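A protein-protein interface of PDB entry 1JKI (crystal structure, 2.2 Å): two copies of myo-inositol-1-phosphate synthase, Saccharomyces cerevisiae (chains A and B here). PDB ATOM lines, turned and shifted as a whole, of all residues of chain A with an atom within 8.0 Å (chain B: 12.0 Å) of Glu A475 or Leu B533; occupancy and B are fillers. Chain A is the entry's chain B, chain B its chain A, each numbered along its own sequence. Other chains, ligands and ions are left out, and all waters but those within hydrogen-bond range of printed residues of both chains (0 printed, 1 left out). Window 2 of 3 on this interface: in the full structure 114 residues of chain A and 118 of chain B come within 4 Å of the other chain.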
ATOM      1  N   GLN A  52       0.490 -10.867  -0.635  1.00  0.00           N
ATOM      2  CA  GLN A  52      -0.375 -11.811   0.062  1.00  0.00           C
ATOM      3  C   GLN A  52       0.509 -12.975   0.492  1.00  0.00           C
ATOM      4  O   GLN A  52       1.260 -13.586  -0.321  1.00  0.00           O
ATOM      5  CB  GLN A  52      -1.454 -12.247  -0.850  1.00  0.00           C
ATOM      6  CG  GLN A  52      -2.282 -13.247  -0.249  1.00  0.00           C
ATOM      7  CD  GLN A  52      -2.677 -12.770   1.102  1.00  0.00           C
ATOM      8  OE1 GLN A  52      -1.888 -12.880   2.008  1.00  0.00           O
ATOM      9  NE2 GLN A  52      -3.858 -12.206   1.234  1.00  0.00           N
ATOM     10  N   TYR A  54       1.027 -16.732   2.127  1.00  0.00           N
ATOM     11  CA  TYR A  54       0.300 -17.999   2.183  1.00  0.00           C
ATOM     12  C   TYR A  54       1.085 -19.050   2.866  1.00  0.00           C
ATOM     13  O   TYR A  54       2.366 -19.025   2.960  1.00  0.00           O
ATOM     14  CB  TYR A  54       0.100 -18.605   0.746  1.00  0.00           C
ATOM     15  CG  TYR A  54      -0.874 -17.835  -0.141  1.00  0.00           C
ATOM     16  CD1 TYR A  54      -0.455 -17.022  -1.160  1.00  0.00           C
ATOM     17  CD2 TYR A  54      -2.196 -17.928   0.083  1.00  0.00           C
ATOM     18  CE1 TYR A  54      -1.393 -16.321  -1.931  1.00  0.00           C
ATOM     19  CE2 TYR A  54      -3.080 -17.254  -0.632  1.00  0.00           C
ATOM     20  CZ  TYR A  54      -2.673 -16.461  -1.629  1.00  0.00           C
ATOM     21  OH  TYR A  54      -3.732 -15.862  -2.238  1.00  0.00           O
ATOM     22  N   VAL A  55       0.281 -20.034   3.308  1.00  0.00           N
ATOM     23  CA  VAL A  55       0.916 -21.275   3.713  1.00  0.00           C
ATOM     24  C   VAL A  55       0.169 -22.375   2.958  1.00  0.00           C
ATOM     25  O   VAL A  55      -1.062 -22.378   2.844  1.00  0.00           O
ATOM     26  CB  VAL A  55       0.922 -21.611   5.228  1.00  0.00           C
ATOM     27  CG1 VAL A  55       2.001 -22.803   5.441  1.00  0.00           C
ATOM     28  CG2 VAL A  55       1.294 -20.297   6.039  1.00  0.00           C
ATOM     29  N   PHE A  56       0.994 -23.257   2.422  1.00  0.00           N
ATOM     30  CA  PHE A  56       0.589 -24.380   1.617  1.00  0.00           C
ATOM     31  C   PHE A  56       0.972 -25.618   2.421  1.00  0.00           C
ATOM     32  O   PHE A  56       2.104 -25.702   2.984  1.00  0.00           O
ATOM     33  CB  PHE A  56       1.394 -24.442   0.255  1.00  0.00           C
ATOM     34  CG  PHE A  56       0.964 -23.403  -0.735  1.00  0.00           C
ATOM     35  CD1 PHE A  56       1.733 -22.244  -0.918  1.00  0.00           C
ATOM     36  CD2 PHE A  56      -0.331 -23.445  -1.243  1.00  0.00           C
ATOM     37  CE1 PHE A  56       1.190 -21.095  -1.553  1.00  0.00           C
ATOM     38  CE2 PHE A  56      -0.886 -22.303  -1.888  1.00  0.00           C
ATOM     39  CZ  PHE A  56      -0.107 -21.103  -2.021  1.00  0.00           C
ATOM     40  N   LYS A  57       0.031 -26.586   2.442  1.00  0.00           N
ATOM     41  CA  LYS A  57       0.257 -27.881   3.149  1.00  0.00           C
ATOM     42  C   LYS A  57       0.057 -28.888   2.023  1.00  0.00           C
ATOM     43  O   LYS A  57      -0.967 -28.896   1.319  1.00  0.00           O
ATOM     44  CB  LYS A  57      -0.813 -28.066   4.245  1.00  0.00           C
ATOM     45  CG  LYS A  57      -0.678 -29.416   5.003  1.00  0.00           C
ATOM     46  CD  LYS A  57      -1.723 -29.502   6.051  1.00  0.00           C
ATOM     47  CE  LYS A  57      -3.059 -28.975   5.524  1.00  0.00           C
ATOM     48  NZ  LYS A  57      -4.080 -29.006   6.722  1.00  0.00           N
ATOM     49  N   CYS A 456      -2.629 -32.025  -7.046  1.00  0.00           N
ATOM     50  CA  CYS A 456      -3.332 -30.920  -6.511  1.00  0.00           C
ATOM     51  C   CYS A 456      -4.166 -31.277  -5.373  1.00  0.00           C
ATOM     52  O   CYS A 456      -4.681 -30.401  -4.574  1.00  0.00           O
ATOM     53  CB  CYS A 456      -4.255 -30.257  -7.560  1.00  0.00           C
ATOM     54  SG  CYS A 456      -3.079 -29.246  -8.722  1.00  0.00           S
ATOM     55  N   VAL A 459      -2.765 -30.903  -1.768  1.00  0.00           N
ATOM     56  CA  VAL A 459      -2.224 -29.613  -1.554  1.00  0.00           C
ATOM     57  C   VAL A 459      -3.282 -28.835  -1.036  1.00  0.00           C
ATOM     58  O   VAL A 459      -4.355 -28.889  -1.640  1.00  0.00           O
ATOM     59  CB  VAL A 459      -1.875 -28.724  -2.865  1.00  0.00           C
ATOM     60  CG1 VAL A 459      -1.761 -27.258  -2.459  1.00  0.00           C
ATOM     61  CG2 VAL A 459      -0.574 -29.213  -3.521  1.00  0.00           C
ATOM     62  N   SER A 460      -3.008 -28.168   0.096  1.00  0.00           N
ATOM     63  CA  SER A 460      -4.006 -27.198   0.620  1.00  0.00           C
ATOM     64  C   SER A 460      -3.251 -25.843   1.000  1.00  0.00           C
ATOM     65  O   SER A 460      -2.010 -25.770   1.115  1.00  0.00           O
ATOM     66  CB  SER A 460      -4.875 -27.801   1.845  1.00  0.00           C
ATOM     67  OG  SER A 460      -4.105 -28.660   2.718  1.00  0.00           O
ATOM     68  N   TYR A 461      -4.020 -24.804   1.251  1.00  0.00           N
ATOM     69  CA  TYR A 461      -3.385 -23.510   1.539  1.00  0.00           C
ATOM     70  C   TYR A 461      -4.121 -22.619   2.589  1.00  0.00           C
ATOM     71  O   TYR A 461      -5.296 -22.774   2.854  1.00  0.00           O
ATOM     72  CB  TYR A 461      -3.336 -22.658   0.191  1.00  0.00           C
ATOM     73  CG  TYR A 461      -4.691 -22.083  -0.248  1.00  0.00           C
ATOM     74  CD1 TYR A 461      -5.037 -20.807   0.043  1.00  0.00           C
ATOM     75  CD2 TYR A 461      -5.611 -22.836  -0.944  1.00  0.00           C
ATOM     76  CE1 TYR A 461      -6.284 -20.276  -0.335  1.00  0.00           C
ATOM     77  CE2 TYR A 461      -6.870 -22.320  -1.347  1.00  0.00           C
ATOM     78  CZ  TYR A 461      -7.200 -21.020  -1.019  1.00  0.00           C
ATOM     79  OH  TYR A 461      -8.502 -20.442  -1.320  1.00  0.00           O
ATOM     80  N   LYS A 462      -3.381 -21.625   3.116  1.00  0.00           N
ATOM     81  CA  LYS A 462      -4.031 -20.588   3.977  1.00  0.00           C
ATOM     82  C   LYS A 462      -3.398 -19.273   3.712  1.00  0.00           C
ATOM     83  O   LYS A 462      -2.156 -19.167   3.570  1.00  0.00           O
ATOM     84  CB  LYS A 462      -4.014 -20.850   5.526  1.00  0.00           C
ATOM     85  CG  LYS A 462      -2.681 -21.155   6.193  1.00  0.00           C
ATOM     86  CD  LYS A 462      -2.886 -21.113   7.727  1.00  0.00           C
ATOM     87  CE  LYS A 462      -1.543 -21.066   8.480  1.00  0.00           C
ATOM     88  NZ  LYS A 462      -1.633 -21.889   9.797  1.00  0.00           N
ATOM     89  N   LYS A 463      -4.305 -18.329   3.567  1.00  0.00           N
ATOM     90  CA  LYS A 463      -3.977 -16.930   3.409  1.00  0.00           C
ATOM     91  C   LYS A 463      -3.517 -16.434   4.794  1.00  0.00           C
ATOM     92  O   LYS A 463      -4.329 -16.347   5.664  1.00  0.00           O
ATOM     93  CB  LYS A 463      -5.236 -16.135   3.073  1.00  0.00           C
ATOM     94  CG  LYS A 463      -5.219 -15.419   1.749  1.00  0.00           C
ATOM     95  CD  LYS A 463      -6.617 -15.012   1.394  1.00  0.00           C
ATOM     96  CE  LYS A 463      -6.761 -14.661  -0.099  1.00  0.00           C
ATOM     97  NZ  LYS A 463      -8.261 -14.273  -0.422  1.00  0.00           N
ATOM     98  N   GLY A 472      -5.935 -20.299  12.232  1.00  0.00           N
ATOM     99  CA  GLY A 472      -5.480 -21.390  11.359  1.00  0.00           C
ATOM    100  C   GLY A 472      -6.359 -21.555  10.120  1.00  0.00           C
ATOM    101  O   GLY A 472      -6.860 -20.597   9.486  1.00  0.00           O
ATOM    102  N   LYS A 473      -6.554 -22.834   9.836  1.00  0.00           N
ATOM    103  CA  LYS A 473      -7.337 -23.473   8.740  1.00  0.00           C
ATOM    104  C   LYS A 473      -7.188 -23.344   7.233  1.00  0.00           C
ATOM    105  O   LYS A 473      -7.770 -22.522   6.542  1.00  0.00           O
ATOM    106  CB  LYS A 473      -8.857 -23.481   8.975  1.00  0.00           C
ATOM    107  CG  LYS A 473      -9.554 -24.514   7.957  1.00  0.00           C
ATOM    108  CD  LYS A 473      -9.069 -26.081   7.967  1.00  0.00           C
ATOM    109  CE  LYS A 473      -7.504 -26.366   8.241  1.00  0.00           C
ATOM    110  NZ  LYS A 473      -6.969 -27.768   8.088  1.00  0.00           N
ATOM    111  N   PHE A 474      -6.448 -24.334   6.777  1.00  0.00           N
ATOM    112  CA  PHE A 474      -6.208 -24.557   5.436  1.00  0.00           C
ATOM    113  C   PHE A 474      -7.510 -24.795   4.737  1.00  0.00           C
ATOM    114  O   PHE A 474      -8.523 -25.162   5.302  1.00  0.00           O
ATOM    115  CB  PHE A 474      -5.351 -25.738   5.333  1.00  0.00           C
ATOM    116  CG  PHE A 474      -4.021 -25.500   5.830  1.00  0.00           C
ATOM    117  CD1 PHE A 474      -3.707 -25.732   7.155  1.00  0.00           C
ATOM    118  CD2 PHE A 474      -3.060 -25.037   4.996  1.00  0.00           C
ATOM    119  CE1 PHE A 474      -2.407 -25.510   7.639  1.00  0.00           C
ATOM    120  CE2 PHE A 474      -1.775 -24.804   5.435  1.00  0.00           C
ATOM    121  CZ  PHE A 474      -1.426 -25.043   6.762  1.00  0.00           C
ATOM    122  N   GLU A 475      -7.463 -24.518   3.442  1.00  0.00           N
ATOM    123  CA  GLU A 475      -8.589 -24.686   2.553  1.00  0.00           C
ATOM    124  C   GLU A 475      -8.068 -25.379   1.296  1.00  0.00           C
ATOM    125  O   GLU A 475      -6.828 -25.497   1.035  1.00  0.00           O
ATOM    126  CB  GLU A 475      -9.206 -23.325   2.269  1.00  0.00           C
ATOM    127  CG  GLU A 475     -10.709 -23.330   2.192  1.00  0.00           C
ATOM    128  CD  GLU A 475     -11.201 -22.049   1.481  1.00  0.00           C
ATOM    129  OE1 GLU A 475     -12.415 -21.911   1.073  1.00  0.00           O
ATOM    130  OE2 GLU A 475     -10.313 -21.147   1.333  1.00  0.00           O
ATOM    131  N   ASN A 476      -9.033 -25.946   0.585  1.00  0.00           N
ATOM    132  CA  ASN A 476      -8.758 -26.620  -0.696  1.00  0.00           C
ATOM    133  C   ASN A 476      -8.685 -25.601  -1.897  1.00  0.00           C
ATOM    134  O   ASN A 476      -9.281 -24.503  -1.875  1.00  0.00           O
ATOM    135  CB  ASN A 476      -9.856 -27.623  -0.968  1.00  0.00           C
ATOM    136  CG  ASN A 476      -9.477 -28.974  -0.560  1.00  0.00           C
ATOM    137  OD1 ASN A 476      -8.285 -29.288  -0.396  1.00  0.00           O
ATOM    138  ND2 ASN A 476     -10.473 -29.819  -0.391  1.00  0.00           N
ATOM    139  N   PHE A 477      -7.895 -25.953  -2.898  1.00  0.00           N
ATOM    140  CA  PHE A 477      -7.831 -25.177  -4.175  1.00  0.00           C
ATOM    141  C   PHE A 477      -9.232 -24.702  -4.586  1.00  0.00           C
ATOM    142  O   PHE A 477     -10.202 -25.439  -4.289  1.00  0.00           O
ATOM    143  CB  PHE A 477      -7.442 -26.142  -5.292  1.00  0.00           C
ATOM    144  CG  PHE A 477      -6.002 -26.273  -5.464  1.00  0.00           C
ATOM    145  CD1 PHE A 477      -5.501 -27.150  -6.382  1.00  0.00           C
ATOM    146  CD2 PHE A 477      -5.142 -25.367  -4.818  1.00  0.00           C
ATOM    147  CE1 PHE A 477      -4.140 -27.155  -6.718  1.00  0.00           C
ATOM    148  CE2 PHE A 477      -3.754 -25.335  -5.131  1.00  0.00           C
ATOM    149  CZ  PHE A 477      -3.242 -26.248  -6.110  1.00  0.00           C
ATOM    150  N   TYR A 478      -9.416 -23.548  -5.244  1.00  0.00           N
ATOM    151  CA  TYR A 478     -10.805 -23.300  -5.742  1.00  0.00           C
ATOM    152  C   TYR A 478     -11.208 -24.642  -6.629  1.00  0.00           C
ATOM    153  O   TYR A 478     -10.310 -25.140  -7.413  1.00  0.00           O
ATOM    154  CB  TYR A 478     -10.781 -22.050  -6.668  1.00  0.00           C
ATOM    155  CG  TYR A 478     -12.126 -21.759  -7.287  1.00  0.00           C
ATOM    156  CD1 TYR A 478     -13.236 -21.673  -6.473  1.00  0.00           C
ATOM    157  CD2 TYR A 478     -12.286 -21.514  -8.658  1.00  0.00           C
ATOM    158  CE1 TYR A 478     -14.472 -21.340  -6.966  1.00  0.00           C
ATOM    159  CE2 TYR A 478     -13.556 -21.168  -9.175  1.00  0.00           C
ATOM    160  CZ  TYR A 478     -14.637 -21.078  -8.284  1.00  0.00           C
ATOM    161  OH  TYR A 478     -15.900 -20.634  -8.618  1.00  0.00           O
ATOM    162  N   PRO A 479     -12.467 -25.259  -6.467  1.00  0.00           N
ATOM    163  CA  PRO A 479     -12.910 -26.463  -7.238  1.00  0.00           C
ATOM    164  C   PRO A 479     -12.220 -26.483  -8.586  1.00  0.00           C
ATOM    165  O   PRO A 479     -11.334 -27.341  -8.800  1.00  0.00           O
ATOM    166  CB  PRO A 479     -14.417 -26.276  -7.335  1.00  0.00           C
ATOM    167  CG  PRO A 479     -14.714 -25.848  -5.872  1.00  0.00           C
ATOM    168  CD  PRO A 479     -13.504 -24.930  -5.450  1.00  0.00           C
ATOM    169  N   ARG A 494     -13.570 -18.931 -13.172  1.00  0.00           N
ATOM    170  CA  ARG A 494     -14.360 -18.395 -12.051  1.00  0.00           C
ATOM    171  C   ARG A 494     -14.871 -17.118 -12.766  1.00  0.00           C
ATOM    172  O   ARG A 494     -14.071 -16.419 -13.431  1.00  0.00           O
ATOM    173  CB  ARG A 494     -13.454 -18.091 -10.812  1.00  0.00           C
ATOM    174  CG  ARG A 494     -13.853 -16.827  -9.931  1.00  0.00           C
ATOM    175  CD  ARG A 494     -13.594 -16.993  -8.399  1.00  0.00           C
ATOM    176  NE  ARG A 494     -12.305 -17.648  -8.111  1.00  0.00           N
ATOM    177  CZ  ARG A 494     -11.663 -17.624  -6.930  1.00  0.00           C
ATOM    178  NH1 ARG A 494     -12.181 -16.967  -5.884  1.00  0.00           N
ATOM    179  NH2 ARG A 494     -10.491 -18.265  -6.790  1.00  0.00           N
ATOM    180  N   PHE A 497     -13.583 -13.485 -14.707  1.00  0.00           N
ATOM    181  CA  PHE A 497     -12.124 -13.642 -14.803  1.00  0.00           C
ATOM    182  C   PHE A 497     -11.749 -14.089 -16.239  1.00  0.00           C
ATOM    183  O   PHE A 497     -12.409 -14.970 -16.864  1.00  0.00           O
ATOM    184  CB  PHE A 497     -11.662 -14.711 -13.777  1.00  0.00           C
ATOM    185  CG  PHE A 497     -10.930 -14.177 -12.595  1.00  0.00           C
ATOM    186  CD1 PHE A 497      -9.564 -13.858 -12.710  1.00  0.00           C
ATOM    187  CD2 PHE A 497     -11.579 -14.031 -11.362  1.00  0.00           C
ATOM    188  CE1 PHE A 497      -8.828 -13.390 -11.600  1.00  0.00           C
ATOM    189  CE2 PHE A 497     -10.860 -13.561 -10.229  1.00  0.00           C
ATOM    190  CZ  PHE A 497      -9.480 -13.242 -10.358  1.00  0.00           C
ATOM    191  N   ILE B 119      -2.454  -6.459 -13.197  1.00  0.00           N
ATOM    192  CA  ILE B 119      -3.837  -6.661 -13.450  1.00  0.00           C
ATOM    193  C   ILE B 119      -4.666  -5.460 -13.146  1.00  0.00           C
ATOM    194  O   ILE B 119      -4.172  -4.489 -12.582  1.00  0.00           O
ATOM    195  CB  ILE B 119      -4.394  -7.869 -12.676  1.00  0.00           C
ATOM    196  CG1 ILE B 119      -4.193  -7.721 -11.159  1.00  0.00           C
ATOM    197  CG2 ILE B 119      -3.694  -9.161 -13.086  1.00  0.00           C
ATOM    198  CD1 ILE B 119      -4.828  -8.866 -10.356  1.00  0.00           C
ATOM    199  N   ALA B 121      -8.739  -3.774 -11.898  1.00  0.00           N
ATOM    200  CA  ALA B 121      -9.763  -4.089 -10.915  1.00  0.00           C
ATOM    201  C   ALA B 121     -10.167  -5.575 -11.039  1.00  0.00           C
ATOM    202  O   ALA B 121     -10.101  -6.377 -10.063  1.00  0.00           O
ATOM    203  CB  ALA B 121     -10.952  -3.253 -11.168  1.00  0.00           C
ATOM    204  N   GLY B 123      -9.453  -9.178 -12.387  1.00  0.00           N
ATOM    205  CA  GLY B 123      -8.242  -9.967 -12.658  1.00  0.00           C
ATOM    206  C   GLY B 123      -7.611  -9.888 -14.016  1.00  0.00           C
ATOM    207  O   GLY B 123      -6.717 -10.658 -14.276  1.00  0.00           O
ATOM    208  N   LEU B 526       1.366 -17.164 -11.714  1.00  0.00           N
ATOM    209  CA  LEU B 526       0.526 -18.024 -10.858  1.00  0.00           C
ATOM    210  C   LEU B 526      -0.873 -17.634 -10.653  1.00  0.00           C
ATOM    211  O   LEU B 526      -1.654 -18.497 -10.250  1.00  0.00           O
ATOM    212  CB  LEU B 526       1.135 -18.230  -9.488  1.00  0.00           C
ATOM    213  CG  LEU B 526       2.601 -18.633  -9.430  1.00  0.00           C
ATOM    214  CD1 LEU B 526       3.077 -18.121  -8.049  1.00  0.00           C
ATOM    215  CD2 LEU B 526       2.861 -20.177  -9.689  1.00  0.00           C
ATOM    216  N   ARG B 527      -1.223 -16.374 -10.916  1.00  0.00           N
ATOM    217  CA  ARG B 527      -2.557 -15.877 -10.736  1.00  0.00           C
ATOM    218  C   ARG B 527      -3.355 -16.354  -9.561  1.00  0.00           C
ATOM    219  O   ARG B 527      -4.568 -16.660  -9.745  1.00  0.00           O
ATOM    220  CB  ARG B 527      -3.470 -16.105 -11.947  1.00  0.00           C
ATOM    221  CG  ARG B 527      -3.022 -15.508 -13.173  1.00  0.00           C
ATOM    222  CD  ARG B 527      -3.238 -16.406 -14.366  1.00  0.00           C
ATOM    223  NE  ARG B 527      -2.763 -15.647 -15.527  1.00  0.00           N
ATOM    224  CZ  ARG B 527      -3.267 -14.471 -15.914  1.00  0.00           C
ATOM    225  NH1 ARG B 527      -4.288 -13.902 -15.251  1.00  0.00           N
ATOM    226  NH2 ARG B 527      -2.707 -13.850 -16.945  1.00  0.00           N
ATOM    227  N   PHE B 528      -2.780 -16.331  -8.333  1.00  0.00           N
ATOM    228  CA  PHE B 528      -3.544 -16.823  -7.147  1.00  0.00           C
ATOM    229  C   PHE B 528      -4.838 -16.064  -6.817  1.00  0.00           C
ATOM    230  O   PHE B 528      -5.710 -16.555  -6.086  1.00  0.00           O
ATOM    231  CB  PHE B 528      -2.656 -16.873  -5.955  1.00  0.00           C
ATOM    232  CG  PHE B 528      -1.588 -17.902  -6.052  1.00  0.00           C
ATOM    233  CD1 PHE B 528      -1.753 -19.024  -6.879  1.00  0.00           C
ATOM    234  CD2 PHE B 528      -0.495 -17.840  -5.240  1.00  0.00           C
ATOM    235  CE1 PHE B 528      -0.815 -20.085  -6.853  1.00  0.00           C
ATOM    236  CE2 PHE B 528       0.424 -18.843  -5.203  1.00  0.00           C
ATOM    237  CZ  PHE B 528       0.263 -19.999  -6.028  1.00  0.00           C
ATOM    238  N   GLU B 529      -5.045 -14.885  -7.364  1.00  0.00           N
ATOM    239  CA  GLU B 529      -6.279 -14.249  -7.024  1.00  0.00           C
ATOM    240  C   GLU B 529      -7.388 -14.890  -7.842  1.00  0.00           C
ATOM    241  O   GLU B 529      -8.596 -14.646  -7.656  1.00  0.00           O
ATOM    242  CB  GLU B 529      -6.216 -12.690  -7.114  1.00  0.00           C
ATOM    243  CG  GLU B 529      -5.566 -12.010  -8.279  1.00  0.00           C
ATOM    244  CD  GLU B 529      -4.053 -11.941  -8.183  1.00  0.00           C
ATOM    245  OE1 GLU B 529      -3.338 -12.829  -8.759  1.00  0.00           O
ATOM    246  OE2 GLU B 529      -3.542 -10.978  -7.550  1.00  0.00           O
ATOM    247  N   GLU B 530      -7.023 -15.789  -8.726  1.00  0.00           N
ATOM    248  CA  GLU B 530      -8.081 -16.426  -9.529  1.00  0.00           C
ATOM    249  C   GLU B 530      -8.170 -17.895  -9.092  1.00  0.00           C
ATOM    250  O   GLU B 530      -9.241 -18.495  -8.974  1.00  0.00           O
ATOM    251  CB  GLU B 530      -7.711 -16.361 -11.033  1.00  0.00           C
ATOM    252  CG  GLU B 530      -8.834 -16.696 -12.073  1.00  0.00           C
ATOM    253  CD  GLU B 530      -8.800 -18.170 -12.681  1.00  0.00           C
ATOM    254  OE1 GLU B 530      -7.805 -18.595 -13.400  1.00  0.00           O
ATOM    255  OE2 GLU B 530      -9.818 -18.891 -12.415  1.00  0.00           O
ATOM    256  N   ARG B 531      -6.992 -18.433  -8.878  1.00  0.00           N
ATOM    257  CA  ARG B 531      -6.715 -19.805  -8.539  1.00  0.00           C
ATOM    258  C   ARG B 531      -6.958 -20.160  -7.039  1.00  0.00           C
ATOM    259  O   ARG B 531      -6.785 -21.314  -6.631  1.00  0.00           O
ATOM    260  CB  ARG B 531      -5.246 -19.975  -8.957  1.00  0.00           C
ATOM    261  CG  ARG B 531      -4.698 -21.322  -9.264  1.00  0.00           C
ATOM    262  CD  ARG B 531      -3.474 -21.186 -10.198  1.00  0.00           C
ATOM    263  NE  ARG B 531      -3.866 -20.677 -11.524  1.00  0.00           N
ATOM    264  CZ  ARG B 531      -3.055 -20.588 -12.580  1.00  0.00           C
ATOM    265  NH1 ARG B 531      -1.790 -20.967 -12.481  1.00  0.00           N
ATOM    266  NH2 ARG B 531      -3.518 -20.105 -13.735  1.00  0.00           N
ATOM    267  N   LEU B 532      -7.405 -19.202  -6.216  1.00  0.00           N
ATOM    268  CA  LEU B 532      -7.538 -19.487  -4.785  1.00  0.00           C
ATOM    269  C   LEU B 532      -8.742 -18.873  -3.986  1.00  0.00           C
ATOM    270  O   LEU B 532      -9.856 -19.463  -3.869  1.00  0.00           O
ATOM    271  CB  LEU B 532      -6.166 -19.136  -4.122  1.00  0.00           C
ATOM    272  CG  LEU B 532      -5.022 -20.179  -3.936  1.00  0.00           C
ATOM    273  CD1 LEU B 532      -4.943 -21.185  -4.979  1.00  0.00           C
ATOM    274  CD2 LEU B 532      -3.679 -19.471  -3.824  1.00  0.00           C
ATOM    275  N   LEU B 533      -8.464 -17.696  -3.407  1.00  0.00           N
ATOM    276  CA  LEU B 533      -9.373 -16.875  -2.547  1.00  0.00           C
ATOM    277  C   LEU B 533      -9.477 -17.560  -1.178  1.00  0.00           C
ATOM    278  O   LEU B 533      -8.412 -17.840  -0.531  1.00  0.00           O
ATOM    279  CB  LEU B 533     -10.798 -16.712  -3.148  1.00  0.00           C
ATOM    280  CG  LEU B 533     -11.443 -15.300  -3.216  1.00  0.00           C
ATOM    281  CD1 LEU B 533     -13.010 -15.455  -3.047  1.00  0.00           C
ATOM    282  CD2 LEU B 533     -10.856 -14.335  -2.139  1.00  0.00           C
ATOM    283  OXT LEU B 533     -10.647 -17.838  -0.783  1.00  0.00           O
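Of the 11 printed residues of chain B, 7 touch a printed residue of chain A. Printed residues of chain B that touch a printed residue of chain A: Gly B123, Phe B528, Glu B529, Glu B530, Arg B531, Leu B532 and Leu B533. Along chain A the printed residues that touch a printed residue of chain B span positions 54 to 497. Among the printed residues, no Asp or Glu carboxylate lies within 4 Å of a Lys or Arg side-chain nitrogen of the other chain.
The backbone carbonyl oxygen (O) of Tyr A461 sits at hydrogen-bond distance from the backbone NH (N) of Glu A475, at 2.8 Å. The guanidinium group (NH1) of Arg B531 sits close to the backbone carbonyl oxygen (O) of Leu B526, at 3.3 Å.
Among the printed residues, pairs that only touch across the chains: Phe A497 with Glu B530 (3.0 Å), Arg A494 with Leu B533 (3.1 Å), Phe A497 with Glu B529 (3.2 Å), Phe A497 with Gly B123 (3.6 Å), Tyr A478 with Arg B531 (3.7 Å), Tyr A54 with Phe B528 (3.8 Å), Tyr A54 with Leu B532 (3.9 Å), Tyr A478 with Leu B532 (3.9 Å), Phe A56 with Phe B528 (3.9 Å) and Glu A475 with Leu B533 (3.9 Å).
Lys A57 touches none of the printed residues of chain B. No residue of chain B comes within 4 Å of Ser A460. Tyr A461 touches two residues of chain B. Lys A463 touches just one residue of chain B: Leu B533 (3.1 Å). No residue of chain B comes within 4 Å of Phe A474. Glu A475 touches just one residue of chain B: Leu B533 (3.9 Å). No residue of chain B comes within 4 Å of Asn A476. Of the printed residues of chain B, Tyr A478 touches Arg B531 and Leu B532. Printed residues of chain B within 4 Å of Phe A497: Gly B123 (3.6 Å), Glu B529 (3.2 Å) and Glu B530 (3.0 Å). Of the printed residues of chain A, Gly B123 touches Phe A497 (3.6 Å). Of the printed residues of chain A, Glu B530 touches Arg A494 and Phe A497. Printed residues of chain A within 4 Å of Arg B531: Tyr A478 (3.7 Å). Of chain A, only Tyr A461 (2.7 Å), Lys A463 (3.1 Å), Glu A475 (3.9 Å) and Arg A494 (3.1 Å) come within 4 Å of Leu B533. The nearest residue of chain B that does not touch Glu A475 is Leu B532 (5.5 Å). The nearest printed residue of chain A that does not touch Leu B532 is Phe A477 (4.2 Å).
NZ of Lys A463 is in salt-bridge range of O of Leu B533, at 3.6 Å. O of Glu B530 sits at hydrogen-bond distance from NH2 of Arg A494. The chain-end carboxylate (O) of Leu B533 lies within hydrogen-bond range of the side-chain hydroxyl (OH) of Tyr A461 (2.7 Å). The backbone carbonyl oxygen of Leu B532 sits at hydrogen-bond distance from the side-chain hydroxyl of Tyr A461 (3.0 Å). NH2 of Arg A494 is in hydrogen-bond range of O of Leu B532 (3.2 Å).
No position is printed for both chains. Of the 15 pairs that touch across the chains among the printed residues, none has its exchanged pair printed and touching as well.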
